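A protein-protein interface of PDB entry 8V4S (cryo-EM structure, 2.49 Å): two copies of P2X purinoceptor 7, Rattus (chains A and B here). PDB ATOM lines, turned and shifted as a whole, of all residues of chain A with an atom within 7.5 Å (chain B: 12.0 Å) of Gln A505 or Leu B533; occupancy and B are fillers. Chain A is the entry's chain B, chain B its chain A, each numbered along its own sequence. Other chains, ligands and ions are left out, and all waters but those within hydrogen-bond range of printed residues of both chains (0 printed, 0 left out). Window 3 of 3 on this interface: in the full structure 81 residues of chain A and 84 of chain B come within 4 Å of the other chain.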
ATOM      1  N   VAL A 404      29.232  -2.010 -29.352  1.00  0.00           N
ATOM      2  CA  VAL A 404      28.354  -2.162 -28.193  1.00  0.00           C
ATOM      3  C   VAL A 404      28.013  -0.809 -27.583  1.00  0.00           C
ATOM      4  O   VAL A 404      26.954  -0.647 -26.964  1.00  0.00           O
ATOM      5  CB  VAL A 404      28.991  -3.114 -27.160  1.00  0.00           C
ATOM      6  CG1 VAL A 404      30.202  -2.472 -26.500  1.00  0.00           C
ATOM      7  CG2 VAL A 404      27.967  -3.542 -26.124  1.00  0.00           C
ATOM      8  N   ASP A 405      28.888   0.181 -27.747  1.00  0.00           N
ATOM      9  CA  ASP A 405      28.628   1.524 -27.245  1.00  0.00           C
ATOM     10  C   ASP A 405      27.818   2.371 -28.218  1.00  0.00           C
ATOM     11  O   ASP A 405      27.667   3.575 -27.994  1.00  0.00           O
ATOM     12  CB  ASP A 405      29.948   2.230 -26.913  1.00  0.00           C
ATOM     13  CG  ASP A 405      30.777   2.526 -28.144  1.00  0.00           C
ATOM     14  OD1 ASP A 405      30.763   1.707 -29.087  1.00  0.00           O
ATOM     15  OD2 ASP A 405      31.444   3.580 -28.172  1.00  0.00           O
ATOM     16  N   GLN A 478      39.729  -0.128 -27.931  1.00  0.00           N
ATOM     17  CA  GLN A 478      39.195   0.689 -26.851  1.00  0.00           C
ATOM     18  C   GLN A 478      38.640  -0.143 -25.703  1.00  0.00           C
ATOM     19  O   GLN A 478      38.003   0.413 -24.802  1.00  0.00           O
ATOM     20  CB  GLN A 478      38.112   1.626 -27.387  1.00  0.00           C
ATOM     21  CG  GLN A 478      38.632   2.957 -27.912  1.00  0.00           C
ATOM     22  CD  GLN A 478      39.084   2.886 -29.356  1.00  0.00           C
ATOM     23  OE1 GLN A 478      39.822   1.984 -29.745  1.00  0.00           O
ATOM     24  NE2 GLN A 478      38.636   3.841 -30.164  1.00  0.00           N
ATOM     25  N   CYS A 479      38.858  -1.460 -25.712  1.00  0.00           N
ATOM     26  CA  CYS A 479      38.388  -2.327 -24.643  1.00  0.00           C
ATOM     27  C   CYS A 479      39.501  -3.053 -23.903  1.00  0.00           C
ATOM     28  O   CYS A 479      39.294  -3.444 -22.749  1.00  0.00           O
ATOM     29  CB  CYS A 479      37.391  -3.367 -25.185  1.00  0.00           C
ATOM     30  SG  CYS A 479      38.111  -4.692 -26.187  1.00  0.00           S
ATOM     31  N   GLY A 480      40.666  -3.246 -24.521  1.00  0.00           N
ATOM     32  CA  GLY A 480      41.802  -3.848 -23.859  1.00  0.00           C
ATOM     33  C   GLY A 480      41.941  -5.344 -24.035  1.00  0.00           C
ATOM     34  O   GLY A 480      43.036  -5.877 -23.815  1.00  0.00           O
ATOM     35  N   CYS A 499      35.274  -3.808 -30.314  1.00  0.00           N
ATOM     36  CA  CYS A 499      33.862  -3.935 -29.990  1.00  0.00           C
ATOM     37  C   CYS A 499      33.201  -2.606 -29.654  1.00  0.00           C
ATOM     38  O   CYS A 499      31.969  -2.548 -29.582  1.00  0.00           O
ATOM     39  CB  CYS A 499      33.679  -4.899 -28.817  1.00  0.00           C
ATOM     40  SG  CYS A 499      34.519  -4.403 -27.296  1.00  0.00           S
ATOM     41  N   ARG A 500      33.977  -1.548 -29.441  1.00  0.00           N
ATOM     42  CA  ARG A 500      33.437  -0.252 -29.066  1.00  0.00           C
ATOM     43  C   ARG A 500      34.284   0.850 -29.685  1.00  0.00           C
ATOM     44  O   ARG A 500      35.481   0.672 -29.925  1.00  0.00           O
ATOM     45  CB  ARG A 500      33.386  -0.093 -27.541  1.00  0.00           C
ATOM     46  CG  ARG A 500      34.561  -0.744 -26.823  1.00  0.00           C
ATOM     47  CD  ARG A 500      34.559  -0.477 -25.321  1.00  0.00           C
ATOM     48  NE  ARG A 500      33.240  -0.606 -24.709  1.00  0.00           N
ATOM     49  CZ  ARG A 500      32.479   0.423 -24.347  1.00  0.00           C
ATOM     50  NH1 ARG A 500      32.902   1.663 -24.541  1.00  0.00           N
ATOM     51  NH2 ARG A 500      31.293   0.210 -23.794  1.00  0.00           N
ATOM     52  N   LYS A 502      34.493   3.901 -28.144  1.00  0.00           N
ATOM     53  CA  LYS A 502      34.996   4.693 -27.038  1.00  0.00           C
ATOM     54  C   LYS A 502      35.497   3.784 -25.924  1.00  0.00           C
ATOM     55  O   LYS A 502      35.031   2.648 -25.789  1.00  0.00           O
ATOM     56  CB  LYS A 502      33.909   5.628 -26.490  1.00  0.00           C
ATOM     57  CG  LYS A 502      33.444   6.687 -27.479  1.00  0.00           C
ATOM     58  CD  LYS A 502      34.579   7.629 -27.849  1.00  0.00           C
ATOM     59  CE  LYS A 502      34.139   8.659 -28.876  1.00  0.00           C
ATOM     60  NZ  LYS A 502      33.767   8.035 -30.176  1.00  0.00           N
ATOM     61  N   PRO A 503      36.457   4.247 -25.122  1.00  0.00           N
ATOM     62  CA  PRO A 503      36.964   3.417 -24.024  1.00  0.00           C
ATOM     63  C   PRO A 503      35.850   3.005 -23.072  1.00  0.00           C
ATOM     64  O   PRO A 503      34.921   3.769 -22.800  1.00  0.00           O
ATOM     65  CB  PRO A 503      37.976   4.331 -23.330  1.00  0.00           C
ATOM     66  CG  PRO A 503      38.452   5.254 -24.397  1.00  0.00           C
ATOM     67  CD  PRO A 503      37.378   5.350 -25.453  1.00  0.00           C
ATOM     68  N   GLY A 504      35.950   1.778 -22.570  1.00  0.00           N
ATOM     69  CA  GLY A 504      34.952   1.274 -21.647  1.00  0.00           C
ATOM     70  C   GLY A 504      35.078  -0.227 -21.483  1.00  0.00           C
ATOM     71  O   GLY A 504      36.101  -0.821 -21.827  1.00  0.00           O
ATOM     72  N   GLN A 505      34.018  -0.824 -20.946  1.00  0.00           N
ATOM     73  CA  GLN A 505      33.993  -2.263 -20.727  1.00  0.00           C
ATOM     74  C   GLN A 505      33.850  -3.011 -22.048  1.00  0.00           C
ATOM     75  O   GLN A 505      33.302  -2.496 -23.026  1.00  0.00           O
ATOM     76  CB  GLN A 505      32.847  -2.636 -19.786  1.00  0.00           C
ATOM     77  CG  GLN A 505      31.577  -1.832 -20.014  1.00  0.00           C
ATOM     78  CD  GLN A 505      30.479  -2.181 -19.027  1.00  0.00           C
ATOM     79  OE1 GLN A 505      30.402  -3.309 -18.538  1.00  0.00           O
ATOM     80  NE2 GLN A 505      29.625  -1.212 -18.726  1.00  0.00           N
ATOM     81  N   CYS A 506      34.355  -4.239 -22.066  1.00  0.00           N
ATOM     82  CA  CYS A 506      34.303  -5.074 -23.255  1.00  0.00           C
ATOM     83  C   CYS A 506      32.993  -5.850 -23.310  1.00  0.00           C
ATOM     84  O   CYS A 506      32.365  -6.126 -22.285  1.00  0.00           O
ATOM     85  CB  CYS A 506      35.484  -6.045 -23.286  1.00  0.00           C
ATOM     86  SG  CYS A 506      35.551  -7.091 -24.756  1.00  0.00           S
ATOM     87  N   ILE A 507      32.585  -6.197 -24.533  1.00  0.00           N
ATOM     88  CA  ILE A 507      31.372  -6.985 -24.728  1.00  0.00           C
ATOM     89  C   ILE A 507      31.528  -8.378 -24.133  1.00  0.00           C
ATOM     90  O   ILE A 507      30.567  -8.948 -23.602  1.00  0.00           O
ATOM     91  CB  ILE A 507      31.016  -7.038 -26.228  1.00  0.00           C
ATOM     92  CG1 ILE A 507      29.787  -7.912 -26.473  1.00  0.00           C
ATOM     93  CG2 ILE A 507      32.189  -7.540 -27.034  1.00  0.00           C
ATOM     94  CD1 ILE A 507      28.487  -7.206 -26.217  1.00  0.00           C
ATOM     95  N   THR A 508      32.736  -8.945 -24.198  1.00  0.00           N
ATOM     96  CA  THR A 508      32.967 -10.295 -23.701  1.00  0.00           C
ATOM     97  C   THR A 508      32.768 -10.412 -22.195  1.00  0.00           C
ATOM     98  O   THR A 508      32.580 -11.524 -21.692  1.00  0.00           O
ATOM     99  CB  THR A 508      34.378 -10.761 -24.063  1.00  0.00           C
ATOM    100  OG1 THR A 508      35.337  -9.826 -23.553  1.00  0.00           O
ATOM    101  CG2 THR A 508      34.536 -10.867 -25.570  1.00  0.00           C
ATOM    102  N   THR A 509      32.809  -9.295 -21.463  1.00  0.00           N
ATOM    103  CA  THR A 509      32.659  -9.347 -20.014  1.00  0.00           C
ATOM    104  C   THR A 509      31.243  -9.707 -19.586  1.00  0.00           C
ATOM    105  O   THR A 509      31.055 -10.198 -18.468  1.00  0.00           O
ATOM    106  CB  THR A 509      33.056  -8.007 -19.393  1.00  0.00           C
ATOM    107  OG1 THR A 509      32.123  -6.996 -19.796  1.00  0.00           O
ATOM    108  CG2 THR A 509      34.454  -7.608 -19.841  1.00  0.00           C
ATOM    109  N   SER A 510      30.251  -9.471 -20.439  1.00  0.00           N
ATOM    110  CA  SER A 510      28.870  -9.767 -20.086  1.00  0.00           C
ATOM    111  C   SER A 510      28.649 -11.271 -19.967  1.00  0.00           C
ATOM    112  O   SER A 510      29.323 -12.077 -20.613  1.00  0.00           O
ATOM    113  CB  SER A 510      27.916  -9.181 -21.126  1.00  0.00           C
ATOM    114  OG  SER A 510      28.209  -9.671 -22.422  1.00  0.00           O
ATOM    115  N   GLU A 511      27.692 -11.644 -19.114  1.00  0.00           N
ATOM    116  CA  GLU A 511      27.340 -13.054 -18.969  1.00  0.00           C
ATOM    117  C   GLU A 511      26.662 -13.591 -20.223  1.00  0.00           C
ATOM    118  O   GLU A 511      26.726 -14.798 -20.492  1.00  0.00           O
ATOM    119  CB  GLU A 511      26.432 -13.247 -17.754  1.00  0.00           C
ATOM    120  CG  GLU A 511      25.141 -12.448 -17.814  1.00  0.00           C
ATOM    121  CD  GLU A 511      24.222 -12.734 -16.644  1.00  0.00           C
ATOM    122  OE1 GLU A 511      24.576 -13.585 -15.801  1.00  0.00           O
ATOM    123  OE2 GLU A 511      23.142 -12.113 -16.570  1.00  0.00           O
ATOM    124  N   TRP A 556      23.419 -12.741 -32.872  1.00  0.00           N
ATOM    125  CA  TRP A 556      23.048 -11.956 -31.700  1.00  0.00           C
ATOM    126  C   TRP A 556      23.212 -10.463 -31.952  1.00  0.00           C
ATOM    127  O   TRP A 556      22.332  -9.669 -31.604  1.00  0.00           O
ATOM    128  CB  TRP A 556      23.892 -12.407 -30.508  1.00  0.00           C
ATOM    129  CG  TRP A 556      23.782 -11.559 -29.275  1.00  0.00           C
ATOM    130  CD1 TRP A 556      22.700 -10.839 -28.859  1.00  0.00           C
ATOM    131  CD2 TRP A 556      24.801 -11.356 -28.290  1.00  0.00           C
ATOM    132  NE1 TRP A 556      22.986 -10.193 -27.682  1.00  0.00           N
ATOM    133  CE2 TRP A 556      24.269 -10.497 -27.310  1.00  0.00           C
ATOM    134  CE3 TRP A 556      26.114 -11.816 -28.144  1.00  0.00           C
ATOM    135  CZ2 TRP A 556      25.004 -10.089 -26.199  1.00  0.00           C
ATOM    136  CZ3 TRP A 556      26.841 -11.410 -27.043  1.00  0.00           C
ATOM    137  CH2 TRP A 556      26.283 -10.554 -26.084  1.00  0.00           C
ATOM    138  N   ARG A 557      24.323 -10.064 -32.568  1.00  0.00           N
ATOM    139  CA  ARG A 557      24.592  -8.644 -32.766  1.00  0.00           C
ATOM    140  C   ARG A 557      23.990  -8.110 -34.060  1.00  0.00           C
ATOM    141  O   ARG A 557      23.522  -6.968 -34.100  1.00  0.00           O
ATOM    142  CB  ARG A 557      26.100  -8.392 -32.741  1.00  0.00           C
ATOM    143  CG  ARG A 557      26.757  -8.799 -31.436  1.00  0.00           C
ATOM    144  CD  ARG A 557      26.017  -8.216 -30.243  1.00  0.00           C
ATOM    145  NE  ARG A 557      25.953  -6.758 -30.300  1.00  0.00           N
ATOM    146  CZ  ARG A 557      25.043  -6.025 -29.670  1.00  0.00           C
ATOM    147  NH1 ARG A 557      24.110  -6.611 -28.933  1.00  0.00           N
ATOM    148  NH2 ARG A 557      25.061  -4.704 -29.781  1.00  0.00           N
ATOM    149  N   GLN B 524      15.153 -10.279 -17.606  1.00  0.00           N
ATOM    150  CA  GLN B 524      16.499  -9.714 -17.583  1.00  0.00           C
ATOM    151  C   GLN B 524      17.330 -10.218 -18.754  1.00  0.00           C
ATOM    152  O   GLN B 524      18.064  -9.444 -19.380  1.00  0.00           O
ATOM    153  CB  GLN B 524      17.183 -10.042 -16.255  1.00  0.00           C
ATOM    154  CG  GLN B 524      16.736  -9.160 -15.101  1.00  0.00           C
ATOM    155  CD  GLN B 524      17.431  -9.506 -13.799  1.00  0.00           C
ATOM    156  OE1 GLN B 524      18.046 -10.563 -13.673  1.00  0.00           O
ATOM    157  NE2 GLN B 524      17.332  -8.612 -12.822  1.00  0.00           N
ATOM    158  N   LEU B 525      17.231 -11.511 -19.067  1.00  0.00           N
ATOM    159  CA  LEU B 525      17.952 -12.048 -20.219  1.00  0.00           C
ATOM    160  C   LEU B 525      17.444 -11.438 -21.519  1.00  0.00           C
ATOM    161  O   LEU B 525      18.235 -11.113 -22.414  1.00  0.00           O
ATOM    162  CB  LEU B 525      17.831 -13.571 -20.256  1.00  0.00           C
ATOM    163  CG  LEU B 525      18.542 -14.330 -19.133  1.00  0.00           C
ATOM    164  CD1 LEU B 525      18.420 -15.833 -19.333  1.00  0.00           C
ATOM    165  CD2 LEU B 525      20.000 -13.912 -19.045  1.00  0.00           C
ATOM    166  N   LEU B 526      16.126 -11.267 -21.639  1.00  0.00           N
ATOM    167  CA  LEU B 526      15.566 -10.636 -22.829  1.00  0.00           C
ATOM    168  C   LEU B 526      16.061  -9.201 -22.973  1.00  0.00           C
ATOM    169  O   LEU B 526      16.373  -8.752 -24.082  1.00  0.00           O
ATOM    170  CB  LEU B 526      14.038 -10.675 -22.764  1.00  0.00           C
ATOM    171  CG  LEU B 526      13.235 -10.478 -24.051  1.00  0.00           C
ATOM    172  CD1 LEU B 526      11.909 -11.208 -23.946  1.00  0.00           C
ATOM    173  CD2 LEU B 526      13.002  -9.001 -24.335  1.00  0.00           C
ATOM    174  N   LEU B 527      16.136  -8.469 -21.862  1.00  0.00           N
ATOM    175  CA  LEU B 527      16.595  -7.085 -21.909  1.00  0.00           C
ATOM    176  C   LEU B 527      18.081  -7.004 -22.236  1.00  0.00           C
ATOM    177  O   LEU B 527      18.514  -6.102 -22.963  1.00  0.00           O
ATOM    178  CB  LEU B 527      16.292  -6.397 -20.579  1.00  0.00           C
ATOM    179  CG  LEU B 527      16.080  -4.885 -20.611  1.00  0.00           C
ATOM    180  CD1 LEU B 527      15.065  -4.511 -21.676  1.00  0.00           C
ATOM    181  CD2 LEU B 527      15.625  -4.400 -19.245  1.00  0.00           C
ATOM    182  N   LEU B 528      18.880  -7.933 -21.705  1.00  0.00           N
ATOM    183  CA  LEU B 528      20.309  -7.939 -21.991  1.00  0.00           C
ATOM    184  C   LEU B 528      20.620  -8.447 -23.391  1.00  0.00           C
ATOM    185  O   LEU B 528      21.723  -8.207 -23.891  1.00  0.00           O
ATOM    186  CB  LEU B 528      21.055  -8.784 -20.959  1.00  0.00           C
ATOM    187  CG  LEU B 528      21.117  -8.222 -19.540  1.00  0.00           C
ATOM    188  CD1 LEU B 528      21.761  -9.224 -18.599  1.00  0.00           C
ATOM    189  CD2 LEU B 528      21.871  -6.902 -19.526  1.00  0.00           C
ATOM    190  N   TYR B 529      19.687  -9.161 -24.022  1.00  0.00           N
ATOM    191  CA  TYR B 529      19.878  -9.551 -25.416  1.00  0.00           C
ATOM    192  C   TYR B 529      20.006  -8.324 -26.310  1.00  0.00           C
ATOM    193  O   TYR B 529      20.892  -8.255 -27.168  1.00  0.00           O
ATOM    194  CB  TYR B 529      18.720 -10.436 -25.874  1.00  0.00           C
ATOM    195  CG  TYR B 529      18.977 -11.175 -27.168  1.00  0.00           C
ATOM    196  CD1 TYR B 529      19.604 -12.412 -27.171  1.00  0.00           C
ATOM    197  CD2 TYR B 529      18.586 -10.635 -28.385  1.00  0.00           C
ATOM    198  CE1 TYR B 529      19.838 -13.089 -28.351  1.00  0.00           C
ATOM    199  CE2 TYR B 529      18.816 -11.305 -29.570  1.00  0.00           C
ATOM    200  CZ  TYR B 529      19.441 -12.532 -29.546  1.00  0.00           C
ATOM    201  OH  TYR B 529      19.671 -13.204 -30.725  1.00  0.00           O
ATOM    202  N   GLN B 530      19.130  -7.337 -26.116  1.00  0.00           N
ATOM    203  CA  GLN B 530      19.192  -6.120 -26.919  1.00  0.00           C
ATOM    204  C   GLN B 530      20.352  -5.230 -26.493  1.00  0.00           C
ATOM    205  O   GLN B 530      21.070  -4.688 -27.343  1.00  0.00           O
ATOM    206  CB  GLN B 530      17.868  -5.363 -26.820  1.00  0.00           C
ATOM    207  CG  GLN B 530      17.912  -3.950 -27.376  1.00  0.00           C
ATOM    208  CD  GLN B 530      16.571  -3.248 -27.287  1.00  0.00           C
ATOM    209  OE1 GLN B 530      15.525  -3.892 -27.198  1.00  0.00           O
ATOM    210  NE2 GLN B 530      16.594  -1.921 -27.309  1.00  0.00           N
ATOM    211  N   GLU B 531      20.556  -5.066 -25.186  1.00  0.00           N
ATOM    212  CA  GLU B 531      21.603  -4.199 -24.643  1.00  0.00           C
ATOM    213  C   GLU B 531      22.471  -5.023 -23.702  1.00  0.00           C
ATOM    214  O   GLU B 531      22.162  -5.160 -22.511  1.00  0.00           O
ATOM    215  CB  GLU B 531      21.004  -2.989 -23.933  1.00  0.00           C
ATOM    216  CG  GLU B 531      20.102  -2.142 -24.818  1.00  0.00           C
ATOM    217  CD  GLU B 531      19.699  -0.835 -24.164  1.00  0.00           C
ATOM    218  OE1 GLU B 531      20.421  -0.375 -23.253  1.00  0.00           O
ATOM    219  OE2 GLU B 531      18.659  -0.268 -24.561  1.00  0.00           O
ATOM    220  N   PRO B 532      23.566  -5.596 -24.207  1.00  0.00           N
ATOM    221  CA  PRO B 532      24.393  -6.477 -23.365  1.00  0.00           C
ATOM    222  C   PRO B 532      25.014  -5.784 -22.165  1.00  0.00           C
ATOM    223  O   PRO B 532      25.178  -6.419 -21.116  1.00  0.00           O
ATOM    224  CB  PRO B 532      25.468  -6.981 -24.338  1.00  0.00           C
ATOM    225  CG  PRO B 532      24.941  -6.678 -25.707  1.00  0.00           C
ATOM    226  CD  PRO B 532      24.109  -5.456 -25.566  1.00  0.00           C
ATOM    227  N   LEU B 533      25.369  -4.506 -22.283  1.00  0.00           N
ATOM    228  CA  LEU B 533      26.030  -3.766 -21.213  1.00  0.00           C
ATOM    229  C   LEU B 533      25.065  -2.814 -20.515  1.00  0.00           C
ATOM    230  O   LEU B 533      25.435  -1.706 -20.121  1.00  0.00           O
ATOM    231  CB  LEU B 533      27.238  -3.004 -21.749  1.00  0.00           C
ATOM    232  CG  LEU B 533      28.342  -3.843 -22.393  1.00  0.00           C
ATOM    233  CD1 LEU B 533      29.493  -2.957 -22.833  1.00  0.00           C
ATOM    234  CD2 LEU B 533      28.826  -4.919 -21.437  1.00  0.00           C
ATOM    235  N   LEU B 534      23.814  -3.238 -20.361  1.00  0.00           N
ATOM    236  CA  LEU B 534      22.816  -2.412 -19.699  1.00  0.00           C
ATOM    237  C   LEU B 534      23.130  -2.277 -18.213  1.00  0.00           C
ATOM    238  O   LEU B 534      23.570  -3.230 -17.563  1.00  0.00           O
ATOM    239  CB  LEU B 534      21.424  -3.013 -19.887  1.00  0.00           C
ATOM    240  CG  LEU B 534      20.255  -2.217 -19.306  1.00  0.00           C
ATOM    241  CD1 LEU B 534      20.122  -0.868 -19.994  1.00  0.00           C
ATOM    242  CD2 LEU B 534      18.971  -3.011 -19.421  1.00  0.00           C
ATOM    243  N   ALA B 535      22.902  -1.079 -17.677  1.00  0.00           N
ATOM    244  CA  ALA B 535      23.129  -0.810 -16.261  1.00  0.00           C
ATOM    245  C   ALA B 535      21.875  -1.178 -15.479  1.00  0.00           C
ATOM    246  O   ALA B 535      20.827  -0.545 -15.637  1.00  0.00           O
ATOM    247  CB  ALA B 535      23.500   0.654 -16.048  1.00  0.00           C
ATOM    248  N   LEU B 536      21.980  -2.203 -14.634  1.00  0.00           N
ATOM    249  CA  LEU B 536      20.846  -2.679 -13.841  1.00  0.00           C
ATOM    250  C   LEU B 536      20.791  -1.917 -12.515  1.00  0.00           C
ATOM    251  O   LEU B 536      21.029  -2.454 -11.430  1.00  0.00           O
ATOM    252  CB  LEU B 536      20.947  -4.184 -13.622  1.00  0.00           C
ATOM    253  CG  LEU B 536      21.169  -5.036 -14.873  1.00  0.00           C
ATOM    254  CD1 LEU B 536      21.288  -6.507 -14.510  1.00  0.00           C
ATOM    255  CD2 LEU B 536      20.051  -4.817 -15.880  1.00  0.00           C
ATOM    256  N   GLU B 537      20.462  -0.632 -12.623  1.00  0.00           N
ATOM    257  CA  GLU B 537      20.386   0.236 -11.457  1.00  0.00           C
ATOM    258  C   GLU B 537      19.357   1.327 -11.709  1.00  0.00           C
ATOM    259  O   GLU B 537      19.009   1.630 -12.854  1.00  0.00           O
ATOM    260  CB  GLU B 537      21.751   0.852 -11.126  1.00  0.00           C
ATOM    261  N   ALA B 540      14.693   2.911 -13.550  1.00  0.00           N
ATOM    262  CA  ALA B 540      14.430   2.630 -14.957  1.00  0.00           C
ATOM    263  C   ALA B 540      14.392   1.134 -15.234  1.00  0.00           C
ATOM    264  O   ALA B 540      13.719   0.697 -16.176  1.00  0.00           O
ATOM    265  CB  ALA B 540      15.481   3.306 -15.835  1.00  0.00           C
ATOM    266  N   ILE B 541      15.104   0.337 -14.433  1.00  0.00           N
ATOM    267  CA  ILE B 541      15.108  -1.105 -14.651  1.00  0.00           C
ATOM    268  C   ILE B 541      13.716  -1.682 -14.424  1.00  0.00           C
ATOM    269  O   ILE B 541      13.262  -2.542 -15.185  1.00  0.00           O
ATOM    270  CB  ILE B 541      16.170  -1.790 -13.768  1.00  0.00           C
ATOM    271  CG1 ILE B 541      16.219  -3.291 -14.061  1.00  0.00           C
ATOM    272  CG2 ILE B 541      15.912  -1.542 -12.290  1.00  0.00           C
ATOM    273  CD1 ILE B 541      17.254  -4.036 -13.250  1.00  0.00           C
ATOM    274  N   LYS B 544      11.543  -0.755 -17.429  1.00  0.00           N
ATOM    275  CA  LYS B 544      11.868  -1.628 -18.588  1.00  0.00           C
ATOM    276  C   LYS B 544      11.281  -3.019 -18.345  1.00  0.00           C
ATOM    277  O   LYS B 544      10.745  -3.607 -19.303  1.00  0.00           O
ATOM    278  CB  LYS B 544      13.385  -1.716 -18.776  1.00  0.00           C
ATOM    279  CG  LYS B 544      14.054  -0.454 -19.302  1.00  0.00           C
ATOM    280  CD  LYS B 544      13.550  -0.046 -20.668  1.00  0.00           C
ATOM    281  CE  LYS B 544      14.347   1.090 -21.273  1.00  0.00           C
ATOM    282  NZ  LYS B 544      15.773   0.727 -21.442  1.00  0.00           N
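Of the 17 printed residues of chain B, 5 touch a printed residue of chain A. Hydrophobic or aromatic side chains of chain B that line the printed part of chain A: Leu B528, Tyr B529, Pro B532 and Leu B533. Hydrophobic or aromatic side chains of chain A that line the printed part of chain B: Val A404, Ile A507 and Trp A556.
Printed residues of chain B within 4 Å of Gln A505: Leu B533 (3.7 Å). Leu B533 touches just these residues of chain A: Val A404 (3.7 Å), Arg A500 (3.8 Å), Gln A505 (3.7 Å) and Cys A506 (3.8 Å). Of chain B, only Leu B533 comes within 4 Å of Val A404. Of chain B, only Leu B533 (3.8 Å) comes within 4 Å of Cys A506. Of the printed residues of chain B, Ile A507 touches Pro B532. No residue of chain B comes within 4 Å of Thr A509. Of chain B, only Pro B532 comes within 4 Å of Ser A510. Of the printed residues of chain A, Tyr B529 touches Trp A556. Printed residues of chain A within 4 Å of Pro B532: Ile A507, Ser A510, Trp A556 and Arg A557. Printed residues of chain B within 4 Å of Arg A557: Gln B530 and Pro B532. Printed residues of chain A within 4 Å of Leu B528: Glu A511 (3.8 Å). Of the printed residues of chain A, Gln B530 touches Arg A557 (3.9 Å). Leu B536 touches none of the printed residues of chain A. The nearest residue of chain A that does not touch Leu B533 is Thr A509 (4.2 Å).
The backbone carbonyl oxygen of Tyr B529 lies within hydrogen-bond range of the indole nitrogen of Trp A556 (2.9 Å).
No position is printed for both chains.
The backbone NH (N) of Val A404 is in hydrogen-bond range of the backbone carbonyl oxygen (O) of Cys A499 (2.8 Å). NH1 of Arg A500 is in hydrogen-bond range of O of Pro A503, at 3.4 Å. The guanidinium group (NE) of Arg A500 lies within hydrogen-bond range of the backbone carbonyl oxygen (O) of Gln A505. The side-chain sulfur (SG) of Cys A506 lies close to the side-chain hydroxyl (OG1) of Thr A508. The side-chain hydroxyl (OG1) of Thr A509 is in hydrogen-bond range of the backbone carbonyl oxygen (O) of Cys A506 (2.6 Å). O of Ile A507 sits at hydrogen-bond distance from OG of Ser A510 (2.7 Å).
Among the printed residues, pairs that only touch across the chains: Arg A557 with Pro B532 (3.3 Å), Trp A556 with Pro B532 (3.4 Å), Ile A507 with Pro B532 (3.6 Å), Gln A505 with Leu B533 (3.7 Å), Val A404 with Leu B533 (3.7 Å), Arg A500 with Leu B533 (3.8 Å), Glu A511 with Leu B528 (3.8 Å), Cys A506 with Leu B533 (3.8 Å), Ser A510 with Pro B532 (3.9 Å) and Arg A557 with Gln B530 (3.9 Å).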
